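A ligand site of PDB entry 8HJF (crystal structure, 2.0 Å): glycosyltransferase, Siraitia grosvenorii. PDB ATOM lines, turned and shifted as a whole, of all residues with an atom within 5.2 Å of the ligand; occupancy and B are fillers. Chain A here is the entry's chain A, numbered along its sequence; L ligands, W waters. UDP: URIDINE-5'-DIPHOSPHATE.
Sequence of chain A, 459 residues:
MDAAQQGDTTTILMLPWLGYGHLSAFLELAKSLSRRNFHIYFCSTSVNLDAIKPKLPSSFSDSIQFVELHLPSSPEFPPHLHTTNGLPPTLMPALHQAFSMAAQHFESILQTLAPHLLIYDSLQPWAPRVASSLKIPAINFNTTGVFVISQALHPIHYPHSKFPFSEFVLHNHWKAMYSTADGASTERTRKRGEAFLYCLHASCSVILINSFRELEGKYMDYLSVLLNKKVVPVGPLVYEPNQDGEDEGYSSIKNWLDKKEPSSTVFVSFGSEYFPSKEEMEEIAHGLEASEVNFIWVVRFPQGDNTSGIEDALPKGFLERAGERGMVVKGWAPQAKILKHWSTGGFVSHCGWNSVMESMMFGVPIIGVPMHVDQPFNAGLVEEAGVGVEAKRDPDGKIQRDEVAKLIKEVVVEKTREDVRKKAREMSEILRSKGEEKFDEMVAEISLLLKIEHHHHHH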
ATOM      1  N   TYR A  20      -5.911  27.815 -14.997  1.00  0.00           N
ATOM      2  CA  TYR A  20      -5.237  28.454 -13.857  1.00  0.00           C
ATOM      3  C   TYR A  20      -3.720  28.301 -13.946  1.00  0.00           C
ATOM      4  O   TYR A  20      -2.982  29.219 -13.567  1.00  0.00           O
ATOM      5  CB  TYR A  20      -5.752  27.872 -12.541  1.00  0.00           C
ATOM      6  CG  TYR A  20      -5.065  28.481 -11.336  1.00  0.00           C
ATOM      7  CD1 TYR A  20      -5.551  29.634 -10.746  1.00  0.00           C
ATOM      8  CD2 TYR A  20      -3.910  27.895 -10.803  1.00  0.00           C
ATOM      9  CE1 TYR A  20      -4.914  30.215  -9.650  1.00  0.00           C
ATOM     10  CE2 TYR A  20      -3.268  28.458  -9.719  1.00  0.00           C
ATOM     11  CZ  TYR A  20      -3.773  29.610  -9.144  1.00  0.00           C
ATOM     12  OH  TYR A  20      -3.128  30.160  -8.063  1.00  0.00           O
ATOM     13  N   GLY A  21      -3.239  27.142 -14.405  1.00  0.00           N
ATOM     14  CA  GLY A  21      -1.806  26.969 -14.579  1.00  0.00           C
ATOM     15  C   GLY A  21      -1.229  27.861 -15.653  1.00  0.00           C
ATOM     16  O   GLY A  21      -0.058  28.249 -15.573  1.00  0.00           O
ATOM     17  N   HIS A  22      -2.016  28.190 -16.660  1.00  0.00           N
ATOM     18  CA  HIS A  22      -1.538  29.100 -17.691  1.00  0.00           C
ATOM     19  C   HIS A  22      -1.497  30.523 -17.161  1.00  0.00           C
ATOM     20  O   HIS A  22      -0.513  31.249 -17.362  1.00  0.00           O
ATOM     21  CB  HIS A  22      -2.417  28.982 -18.940  1.00  0.00           C
ATOM     22  CG  HIS A  22      -2.407  27.624 -19.556  1.00  0.00           C
ATOM     23  ND1 HIS A  22      -1.893  27.386 -20.817  1.00  0.00           N
ATOM     24  CD2 HIS A  22      -2.801  26.415 -19.073  1.00  0.00           C
ATOM     25  CE1 HIS A  22      -1.995  26.090 -21.093  1.00  0.00           C
ATOM     26  NE2 HIS A  22      -2.542  25.478 -20.056  1.00  0.00           N
ATOM     27  N   SER A  24      -0.966  31.301 -14.117  1.00  0.00           N
ATOM     28  CA  SER A  24       0.137  31.402 -13.168  1.00  0.00           C
ATOM     29  C   SER A  24       1.468  31.653 -13.865  1.00  0.00           C
ATOM     30  O   SER A  24       2.193  32.589 -13.510  1.00  0.00           O
ATOM     31  CB  SER A  24       0.221  30.130 -12.299  1.00  0.00           C
ATOM     32  OG  SER A  24      -1.027  29.846 -11.685  1.00  0.00           O
ATOM     33  N   LYS A  55      -1.779  36.232  -6.123  1.00  0.00           N
ATOM     34  CA  LYS A  55      -0.391  35.925  -6.426  1.00  0.00           C
ATOM     35  C   LYS A  55       0.393  37.138  -6.913  1.00  0.00           C
ATOM     36  O   LYS A  55       1.578  37.009  -7.248  1.00  0.00           O
ATOM     37  CB  LYS A  55      -0.302  34.808  -7.477  1.00  0.00           C
ATOM     38  CG  LYS A  55      -0.664  33.441  -6.934  1.00  0.00           C
ATOM     39  CD  LYS A  55      -0.543  32.366  -8.003  1.00  0.00           C
ATOM     40  CE  LYS A  55       0.087  31.107  -7.452  1.00  0.00           C
ATOM     41  NZ  LYS A  55      -0.913  30.090  -7.021  1.00  0.00           N
ATOM     42  N   PHE A 267       2.677  15.844  -0.018  1.00  0.00           N
ATOM     43  CA  PHE A 267       1.557  16.590  -0.553  1.00  0.00           C
ATOM     44  C   PHE A 267       0.995  15.835  -1.747  1.00  0.00           C
ATOM     45  O   PHE A 267       1.747  15.212  -2.507  1.00  0.00           O
ATOM     46  CB  PHE A 267       2.006  17.994  -0.962  1.00  0.00           C
ATOM     47  CG  PHE A 267       0.890  18.888  -1.428  1.00  0.00           C
ATOM     48  CD1 PHE A 267      -0.179  19.174  -0.592  1.00  0.00           C
ATOM     49  CD2 PHE A 267       0.916  19.445  -2.700  1.00  0.00           C
ATOM     50  CE1 PHE A 267      -1.201  20.004  -1.018  1.00  0.00           C
ATOM     51  CE2 PHE A 267      -0.104  20.271  -3.134  1.00  0.00           C
ATOM     52  CZ  PHE A 267      -1.164  20.559  -2.298  1.00  0.00           C
ATOM     53  N   SER A 269      -1.806  16.219  -4.938  1.00  0.00           N
ATOM     54  CA  SER A 269      -2.630  17.154  -5.689  1.00  0.00           C
ATOM     55  C   SER A 269      -2.581  16.793  -7.160  1.00  0.00           C
ATOM     56  O   SER A 269      -1.557  16.326  -7.670  1.00  0.00           O
ATOM     57  CB  SER A 269      -2.168  18.599  -5.481  1.00  0.00           C
ATOM     58  OG  SER A 269      -3.040  19.501  -6.152  1.00  0.00           O
ATOM     59  N   PHE A 270      -3.700  17.023  -7.846  1.00  0.00           N
ATOM     60  CA  PHE A 270      -3.796  16.749  -9.263  1.00  0.00           C
ATOM     61  C   PHE A 270      -4.161  18.019 -10.042  1.00  0.00           C
ATOM     62  O   PHE A 270      -4.732  17.954 -11.127  1.00  0.00           O
ATOM     63  CB  PHE A 270      -4.789  15.613  -9.507  1.00  0.00           C
ATOM     64  CG  PHE A 270      -4.390  14.346  -8.794  1.00  0.00           C
ATOM     65  CD1 PHE A 270      -3.425  13.514  -9.341  1.00  0.00           C
ATOM     66  CD2 PHE A 270      -4.896  14.056  -7.548  1.00  0.00           C
ATOM     67  CE1 PHE A 270      -3.021  12.365  -8.671  1.00  0.00           C
ATOM     68  CE2 PHE A 270      -4.503  12.912  -6.883  1.00  0.00           C
ATOM     69  CZ  PHE A 270      -3.556  12.072  -7.439  1.00  0.00           C
ATOM     70  N   GLY A 271      -3.792  19.169  -9.486  1.00  0.00           N
ATOM     71  CA  GLY A 271      -3.837  20.422 -10.222  1.00  0.00           C
ATOM     72  C   GLY A 271      -5.199  21.081 -10.227  1.00  0.00           C
ATOM     73  O   GLY A 271      -6.068  20.844  -9.365  1.00  0.00           O
ATOM     74  N   SER A 272      -5.401  21.912 -11.241  1.00  0.00           N
ATOM     75  CA  SER A 272      -6.549  22.813 -11.287  1.00  0.00           C
ATOM     76  C   SER A 272      -7.718  22.305 -12.124  1.00  0.00           C
ATOM     77  O   SER A 272      -8.850  22.768 -11.921  1.00  0.00           O
ATOM     78  CB  SER A 272      -6.123  24.171 -11.848  1.00  0.00           C
ATOM     79  OG  SER A 272      -5.898  24.106 -13.258  1.00  0.00           O
ATOM     80  N   GLU A 273      -7.490  21.357 -13.036  1.00  0.00           N
ATOM     81  CA  GLU A 273      -8.505  21.020 -14.034  1.00  0.00           C
ATOM     82  C   GLU A 273      -8.552  19.514 -14.263  1.00  0.00           C
ATOM     83  O   GLU A 273      -8.606  19.039 -15.398  1.00  0.00           O
ATOM     84  CB  GLU A 273      -8.233  21.763 -15.333  1.00  0.00           C
ATOM     85  CG  GLU A 273      -6.761  21.941 -15.627  1.00  0.00           C
ATOM     86  CD  GLU A 273      -6.470  22.312 -17.061  1.00  0.00           C
ATOM     87  OE1 GLU A 273      -6.668  23.486 -17.443  1.00  0.00           O
ATOM     88  OE2 GLU A 273      -6.036  21.425 -17.821  1.00  0.00           O
ATOM     89  N   VAL A 298      -5.308  17.217  -1.483  1.00  0.00           N
ATOM     90  CA  VAL A 298      -6.299  18.159  -1.989  1.00  0.00           C
ATOM     91  C   VAL A 298      -7.336  17.377  -2.775  1.00  0.00           C
ATOM     92  O   VAL A 298      -7.002  16.696  -3.750  1.00  0.00           O
ATOM     93  CB  VAL A 298      -5.663  19.248  -2.872  1.00  0.00           C
ATOM     94  CG1 VAL A 298      -6.734  20.180  -3.387  1.00  0.00           C
ATOM     95  CG2 VAL A 298      -4.620  20.007  -2.107  1.00  0.00           C
ATOM     96  N   GLY A 331     -11.049  21.522  -1.974  1.00  0.00           N
ATOM     97  CA  GLY A 331     -11.017  22.653  -2.882  1.00  0.00           C
ATOM     98  C   GLY A 331      -9.641  23.101  -3.322  1.00  0.00           C
ATOM     99  O   GLY A 331      -9.284  22.950  -4.486  1.00  0.00           O
ATOM    100  N   TRP A 332      -8.843  23.647  -2.398  1.00  0.00           N
ATOM    101  CA  TRP A 332      -7.617  24.337  -2.780  1.00  0.00           C
ATOM    102  C   TRP A 332      -6.680  24.391  -1.578  1.00  0.00           C
ATOM    103  O   TRP A 332      -7.147  24.538  -0.443  1.00  0.00           O
ATOM    104  CB  TRP A 332      -7.935  25.743  -3.267  1.00  0.00           C
ATOM    105  CG  TRP A 332      -6.850  26.374  -4.058  1.00  0.00           C
ATOM    106  CD1 TRP A 332      -5.939  27.288  -3.623  1.00  0.00           C
ATOM    107  CD2 TRP A 332      -6.564  26.128  -5.436  1.00  0.00           C
ATOM    108  NE1 TRP A 332      -5.097  27.636  -4.646  1.00  0.00           N
ATOM    109  CE2 TRP A 332      -5.449  26.938  -5.777  1.00  0.00           C
ATOM    110  CE3 TRP A 332      -7.132  25.308  -6.421  1.00  0.00           C
ATOM    111  CZ2 TRP A 332      -4.909  26.949  -7.047  1.00  0.00           C
ATOM    112  CZ3 TRP A 332      -6.584  25.326  -7.681  1.00  0.00           C
ATOM    113  CH2 TRP A 332      -5.479  26.132  -7.987  1.00  0.00           C
ATOM    114  N   ALA A 333      -5.385  24.301  -1.823  1.00  0.00           N
ATOM    115  CA  ALA A 333      -4.387  24.341  -0.765  1.00  0.00           C
ATOM    116  C   ALA A 333      -3.252  25.293  -1.113  1.00  0.00           C
ATOM    117  O   ALA A 333      -2.992  25.565  -2.288  1.00  0.00           O
ATOM    118  CB  ALA A 333      -3.814  22.940  -0.492  1.00  0.00           C
ATOM    119  N   PRO A 334      -2.574  25.845  -0.098  1.00  0.00           N
ATOM    120  CA  PRO A 334      -1.348  26.603  -0.367  1.00  0.00           C
ATOM    121  C   PRO A 334      -0.204  25.675  -0.759  1.00  0.00           C
ATOM    122  O   PRO A 334       0.623  25.294   0.088  1.00  0.00           O
ATOM    123  CB  PRO A 334      -1.068  27.304   0.971  1.00  0.00           C
ATOM    124  CG  PRO A 334      -1.759  26.474   1.989  1.00  0.00           C
ATOM    125  CD  PRO A 334      -2.974  25.912   1.315  1.00  0.00           C
ATOM    126  N   GLN A 335      -0.143  25.312  -2.041  1.00  0.00           N
ATOM    127  CA  GLN A 335       0.755  24.256  -2.485  1.00  0.00           C
ATOM    128  C   GLN A 335       2.213  24.609  -2.242  1.00  0.00           C
ATOM    129  O   GLN A 335       2.981  23.792  -1.730  1.00  0.00           O
ATOM    130  CB  GLN A 335       0.512  23.963  -3.964  1.00  0.00           C
ATOM    131  CG  GLN A 335       1.666  23.225  -4.635  1.00  0.00           C
ATOM    132  CD  GLN A 335       1.241  22.515  -5.900  1.00  0.00           C
ATOM    133  OE1 GLN A 335       0.076  22.115  -6.042  1.00  0.00           O
ATOM    134  NE2 GLN A 335       2.172  22.365  -6.837  1.00  0.00           N
ATOM    135  N   ALA A 336       2.622  25.827  -2.635  1.00  0.00           N
ATOM    136  CA  ALA A 336       4.028  26.207  -2.509  1.00  0.00           C
ATOM    137  C   ALA A 336       4.477  26.187  -1.049  1.00  0.00           C
ATOM    138  O   ALA A 336       5.510  25.592  -0.708  1.00  0.00           O
ATOM    139  CB  ALA A 336       4.267  27.587  -3.127  1.00  0.00           C
ATOM    140  N   HIS A 350       0.067  14.990 -10.174  1.00  0.00           N
ATOM    141  CA  HIS A 350      -0.332  14.682 -11.545  1.00  0.00           C
ATOM    142  C   HIS A 350       0.716  15.115 -12.556  1.00  0.00           C
ATOM    143  O   HIS A 350       0.616  14.759 -13.731  1.00  0.00           O
ATOM    144  CB  HIS A 350      -1.678  15.337 -11.859  1.00  0.00           C
ATOM    145  CG  HIS A 350      -1.605  16.818 -12.075  1.00  0.00           C
ATOM    146  ND1 HIS A 350      -0.879  17.653 -11.256  1.00  0.00           N
ATOM    147  CD2 HIS A 350      -2.183  17.612 -13.006  1.00  0.00           C
ATOM    148  CE1 HIS A 350      -1.010  18.904 -11.670  1.00  0.00           C
ATOM    149  NE2 HIS A 350      -1.792  18.904 -12.735  1.00  0.00           N
ATOM    150  N   GLY A 352       1.550  18.239 -13.539  1.00  0.00           N
ATOM    151  CA  GLY A 352       1.391  19.487 -14.245  1.00  0.00           C
ATOM    152  C   GLY A 352       2.730  20.196 -14.258  1.00  0.00           C
ATOM    153  O   GLY A 352       3.506  20.017 -13.313  1.00  0.00           O
ATOM    154  N   TRP A 353       3.031  20.979 -15.284  1.00  0.00           N
ATOM    155  CA  TRP A 353       4.384  21.512 -15.416  1.00  0.00           C
ATOM    156  C   TRP A 353       4.695  22.538 -14.337  1.00  0.00           C
ATOM    157  O   TRP A 353       5.835  22.615 -13.855  1.00  0.00           O
ATOM    158  CB  TRP A 353       4.587  22.125 -16.793  1.00  0.00           C
ATOM    159  CG  TRP A 353       6.024  22.459 -17.088  1.00  0.00           C
ATOM    160  CD1 TRP A 353       6.538  23.689 -17.377  1.00  0.00           C
ATOM    161  CD2 TRP A 353       7.118  21.540 -17.134  1.00  0.00           C
ATOM    162  NE1 TRP A 353       7.893  23.602 -17.600  1.00  0.00           N
ATOM    163  CE2 TRP A 353       8.277  22.288 -17.456  1.00  0.00           C
ATOM    164  CE3 TRP A 353       7.248  20.163 -16.929  1.00  0.00           C
ATOM    165  CZ2 TRP A 353       9.544  21.709 -17.581  1.00  0.00           C
ATOM    166  CZ3 TRP A 353       8.505  19.582 -17.055  1.00  0.00           C
ATOM    167  CH2 TRP A 353       9.628  20.354 -17.385  1.00  0.00           C
ATOM    168  N   ASN A 354       3.709  23.362 -13.952  1.00  0.00           N
ATOM    169  CA  ASN A 354       3.937  24.297 -12.859  1.00  0.00           C
ATOM    170  C   ASN A 354       4.262  23.549 -11.569  1.00  0.00           C
ATOM    171  O   ASN A 354       5.162  23.949 -10.824  1.00  0.00           O
ATOM    172  CB  ASN A 354       2.707  25.193 -12.650  1.00  0.00           C
ATOM    173  CG  ASN A 354       2.557  26.253 -13.713  1.00  0.00           C
ATOM    174  OD1 ASN A 354       3.508  26.968 -14.041  1.00  0.00           O
ATOM    175  ND2 ASN A 354       1.341  26.380 -14.242  1.00  0.00           N
ATOM    176  N   SER A 355       3.540  22.468 -11.297  1.00  0.00           N
ATOM    177  CA  SER A 355       3.815  21.650 -10.127  1.00  0.00           C
ATOM    178  C   SER A 355       5.167  20.964 -10.224  1.00  0.00           C
ATOM    179  O   SER A 355       5.816  20.739  -9.195  1.00  0.00           O
ATOM    180  CB  SER A 355       2.718  20.609  -9.920  1.00  0.00           C
ATOM    181  OG  SER A 355       1.450  21.210  -9.679  1.00  0.00           O
ATOM    182  N   VAL A 356       5.597  20.587 -11.434  1.00  0.00           N
ATOM    183  CA  VAL A 356       6.927  20.007 -11.582  1.00  0.00           C
ATOM    184  C   VAL A 356       8.000  21.064 -11.339  1.00  0.00           C
ATOM    185  O   VAL A 356       8.958  20.844 -10.583  1.00  0.00           O
ATOM    186  CB  VAL A 356       7.109  19.361 -12.963  1.00  0.00           C
ATOM    187  CG1 VAL A 356       8.546  18.901 -13.125  1.00  0.00           C
ATOM    188  CG2 VAL A 356       6.152  18.195 -13.171  1.00  0.00           C
ATOM    189  N   GLU A 358       7.760  23.844  -9.671  1.00  0.00           N
ATOM    190  CA  GLU A 358       7.742  24.212  -8.256  1.00  0.00           C
ATOM    191  C   GLU A 358       8.462  23.173  -7.407  1.00  0.00           C
ATOM    192  O   GLU A 358       9.345  23.504  -6.614  1.00  0.00           O
ATOM    193  CB  GLU A 358       6.295  24.384  -7.783  1.00  0.00           C
ATOM    194  CG  GLU A 358       5.638  25.659  -8.278  1.00  0.00           C
ATOM    195  CD  GLU A 358       4.116  25.617  -8.255  1.00  0.00           C
ATOM    196  OE1 GLU A 358       3.538  24.658  -7.689  1.00  0.00           O
ATOM    197  OE2 GLU A 358       3.508  26.555  -8.796  1.00  0.00           O
ATOM    198  N   GLN A 375       0.955  15.589 -19.024  1.00  0.00           N
ATOM    199  CA  GLN A 375       1.484  15.039 -17.787  1.00  0.00           C
ATOM    200  C   GLN A 375       2.297  13.758 -17.968  1.00  0.00           C
ATOM    201  O   GLN A 375       3.349  13.648 -17.316  1.00  0.00           O
ATOM    202  CB  GLN A 375       0.314  14.835 -16.809  1.00  0.00           C
ATOM    203  CG  GLN A 375      -0.305  16.154 -16.371  1.00  0.00           C
ATOM    204  CD  GLN A 375      -1.816  16.090 -16.252  1.00  0.00           C
ATOM    205  OE1 GLN A 375      -2.387  15.053 -15.897  1.00  0.00           O
ATOM    206  NE2 GLN A 375      -2.474  17.194 -16.558  1.00  0.00           N
HETATM  207  N1  UDP L   1      -2.189  24.864  -6.975  1.00  0.00           N
HETATM  208  C2  UDP L   1      -2.420  25.442  -5.751  1.00  0.00           C
HETATM  209  N3  UDP L   1      -3.225  24.738  -4.881  1.00  0.00           N
HETATM  210  C4  UDP L   1      -3.809  23.520  -5.123  1.00  0.00           C
HETATM  211  C5  UDP L   1      -3.517  22.959  -6.416  1.00  0.00           C
HETATM  212  C6  UDP L   1      -2.735  23.631  -7.295  1.00  0.00           C
HETATM  213  O2  UDP L   1      -1.965  26.535  -5.439  1.00  0.00           O
HETATM  214  O4  UDP L   1      -4.507  22.977  -4.255  1.00  0.00           O
HETATM  215  C1' UDP L   1      -1.347  25.564  -7.964  1.00  0.00           C
HETATM  216  C2' UDP L   1       0.006  24.805  -8.182  1.00  0.00           C
HETATM  217  O2' UDP L   1       0.955  25.214  -7.201  1.00  0.00           O
HETATM  218  C3' UDP L   1       0.388  25.269  -9.571  1.00  0.00           C
HETATM  219  C4' UDP L   1      -0.960  25.382 -10.278  1.00  0.00           C
HETATM  220  O4' UDP L   1      -1.986  25.480  -9.236  1.00  0.00           O
HETATM  221  O3' UDP L   1       1.029  26.550  -9.541  1.00  0.00           O
HETATM  222  C5' UDP L   1      -1.227  24.154 -11.096  1.00  0.00           C
HETATM  223  O5' UDP L   1      -0.481  24.191 -12.274  1.00  0.00           O
HETATM  224  PA  UDP L   1      -0.011  22.758 -12.930  1.00  0.00           P
HETATM  225  O1A UDP L   1       0.731  23.011 -14.219  1.00  0.00           O
HETATM  226  O2A UDP L   1       0.876  22.003 -11.978  1.00  0.00           O
HETATM  227  O3A UDP L   1      -1.341  21.845 -13.184  1.00  0.00           O
HETATM  228  PB  UDP L   1      -2.734  22.214 -13.960  1.00  0.00           P
HETATM  229  O1B UDP L   1      -2.450  23.184 -15.083  1.00  0.00           O
HETATM  230  O2B UDP L   1      -3.310  20.933 -14.490  1.00  0.00           O
HETATM  231  O3B UDP L   1      -3.639  22.870 -12.956  1.00  0.00           O
HETATM  232  O   HOH W   1       1.476  27.829  -6.282  1.00  0.00           O
HETATM  233  O   HOH W   2      -1.942  28.699  -3.762  1.00  0.00           O
HETATM  234  O   HOH W   3      -1.269  20.762  -7.978  1.00  0.00           O
HETATM  235  O   HOH W   4      -4.149  25.054 -16.153  1.00  0.00           O
HETATM  236  O   HOH W   5      -3.427  20.106 -16.924  1.00  0.00           O
HETATM  237  O   HOH W   6      -5.443  19.540 -13.478  1.00  0.00           O
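The side-chain amide nitrogen (NE2) of Gln 335 sits close to an oxygen (O2') of the ligand (3.1 Å).
O3B of the ligand is in hydrogen-bond range of OG of Ser 272 (2.6 Å).
The side-chain carboxylate (OE2) of Glu 358 is in hydrogen-bond range of an oxygen (O3') of the ligand (2.6 Å).
The backbone carbonyl oxygen of Ala 333 lies within hydrogen-bond range of a nitrogen (N3) of the ligand, at 2.7 Å.
The side-chain hydroxyl (OG) of Ser 355 lies within hydrogen-bond range of an oxygen (O2A) of the ligand, 2.5 Å away.
The backbone NH (N) of Ser 272 lies within hydrogen-bond range of an oxygen (O3B) of the ligand (2.6 Å).
N of Ala 333 sits at hydrogen-bond distance from O4 of the ligand (2.9 Å).
An oxygen (O2) of the ligand lies close to the indole nitrogen of Trp 332, 3.4 Å away.
The backbone NH (N) of Ser 355 is in hydrogen-bond range of an oxygen (O2A) of the ligand (2.8 Å).
The backbone NH (N) of Trp 353 lies within hydrogen-bond range of an oxygen (O1A) of the ligand, at 3.2 Å.
N of Asn 354 lies within hydrogen-bond range of O1A of the ligand.
A ring nitrogen (NE2) of His 350 is in hydrogen-bond range of an oxygen (O3A) of the ligand, at 3.0 Å.
ND2 of Asn 354 sits close to O1A of the ligand.
The backbone NH (N) of His 350 is in hydrogen-bond range of the backbone carbonyl oxygen (O) of Ser 269 (3.3 Å).
ND1 of His 350 sits close to N of Gly 352, 3.4 Å away.
The side-chain amide nitrogen (ND2) of Asn 354 sits at hydrogen-bond distance from the backbone carbonyl oxygen (O) of Gly 21, at 2.7 Å.
The side-chain carboxylate (OE1) of Glu 358 is in hydrogen-bond range of the side-chain amide nitrogen (NE2) of Gln 335 (2.8 Å).
A ring nitrogen (NE2) of His 350 lies close to the backbone carbonyl oxygen of Phe 270 (3.5 Å).
OG of Ser 24 sits at hydrogen-bond distance from O of Tyr 20 (2.8 Å).
OH of Tyr 20 lies within hydrogen-bond range of NZ of Lys 55, 2.4 Å away.
OG of Ser 355 lies within hydrogen-bond range of NE2 of Gln 335 (3.2 Å).
Residues that only touch the ligand: Tyr 20 (3.3 Å), Gly 21 (3.8 Å), Ser 269 (3.5 Å), Gly 271 (3.6 Å), Glu 273 (3.8 Å), Val 298 (3.7 Å) and Gly 352 (3.4 Å).
Hydrophobic or aromatic side chains within 4 Å of the ligand: Tyr 20, Val 298, Trp 332, Ala 333 and His 350.
16 residues have an atom within 4 Å of the ligand: Tyr 20, Gly 21, Ser 269, Gly 271, Ser 272, Glu 273, Val 298, Trp 332, Ala 333, Gln 335, His 350, Gly 352, Trp 353, Asn 354, Ser 355 and Glu 358.
The nearest printed residue that does not touch the ligand is Lys 55 (4.03 Å).
Water W5 lies within hydrogen-bond range of O2B of the ligand (2.6 Å), OE2 of Glu 273 (3.1 Å) and NE2 of Gln 375 (3.1 Å).
Water W2 bridges O2 of the ligand (2.7 Å) and NE1 of Trp 332 (3.4 Å).
Water W6 lies within hydrogen-bond range of O2B of the ligand (2.7 Å), N of Glu 273 (2.8 Å), O of Phe 270 (2.9 Å) and N of Ser 272 (3.3 Å).
Water W4 lies within hydrogen-bond range of O1B of the ligand (2.7 Å), N of Gly 21 (2.9 Å), OE1 of Glu 273 (3.2 Å) and N of Tyr 20 (3.5 Å).
Water W1 lies within hydrogen-bond range of an oxygen (O2') of the ligand (2.8 Å), the side-chain amino group of Lys 55 (3.4 Å) and the side-chain carboxylate of Glu 358 (3.5 Å).
Water W3 lies within hydrogen-bond range of OE1 of Gln 335 (2.7 Å), OG of Ser 269 (2.8 Å), OG of Ser 355 (3.2 Å) and N of Gly 271 (3.3 Å).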
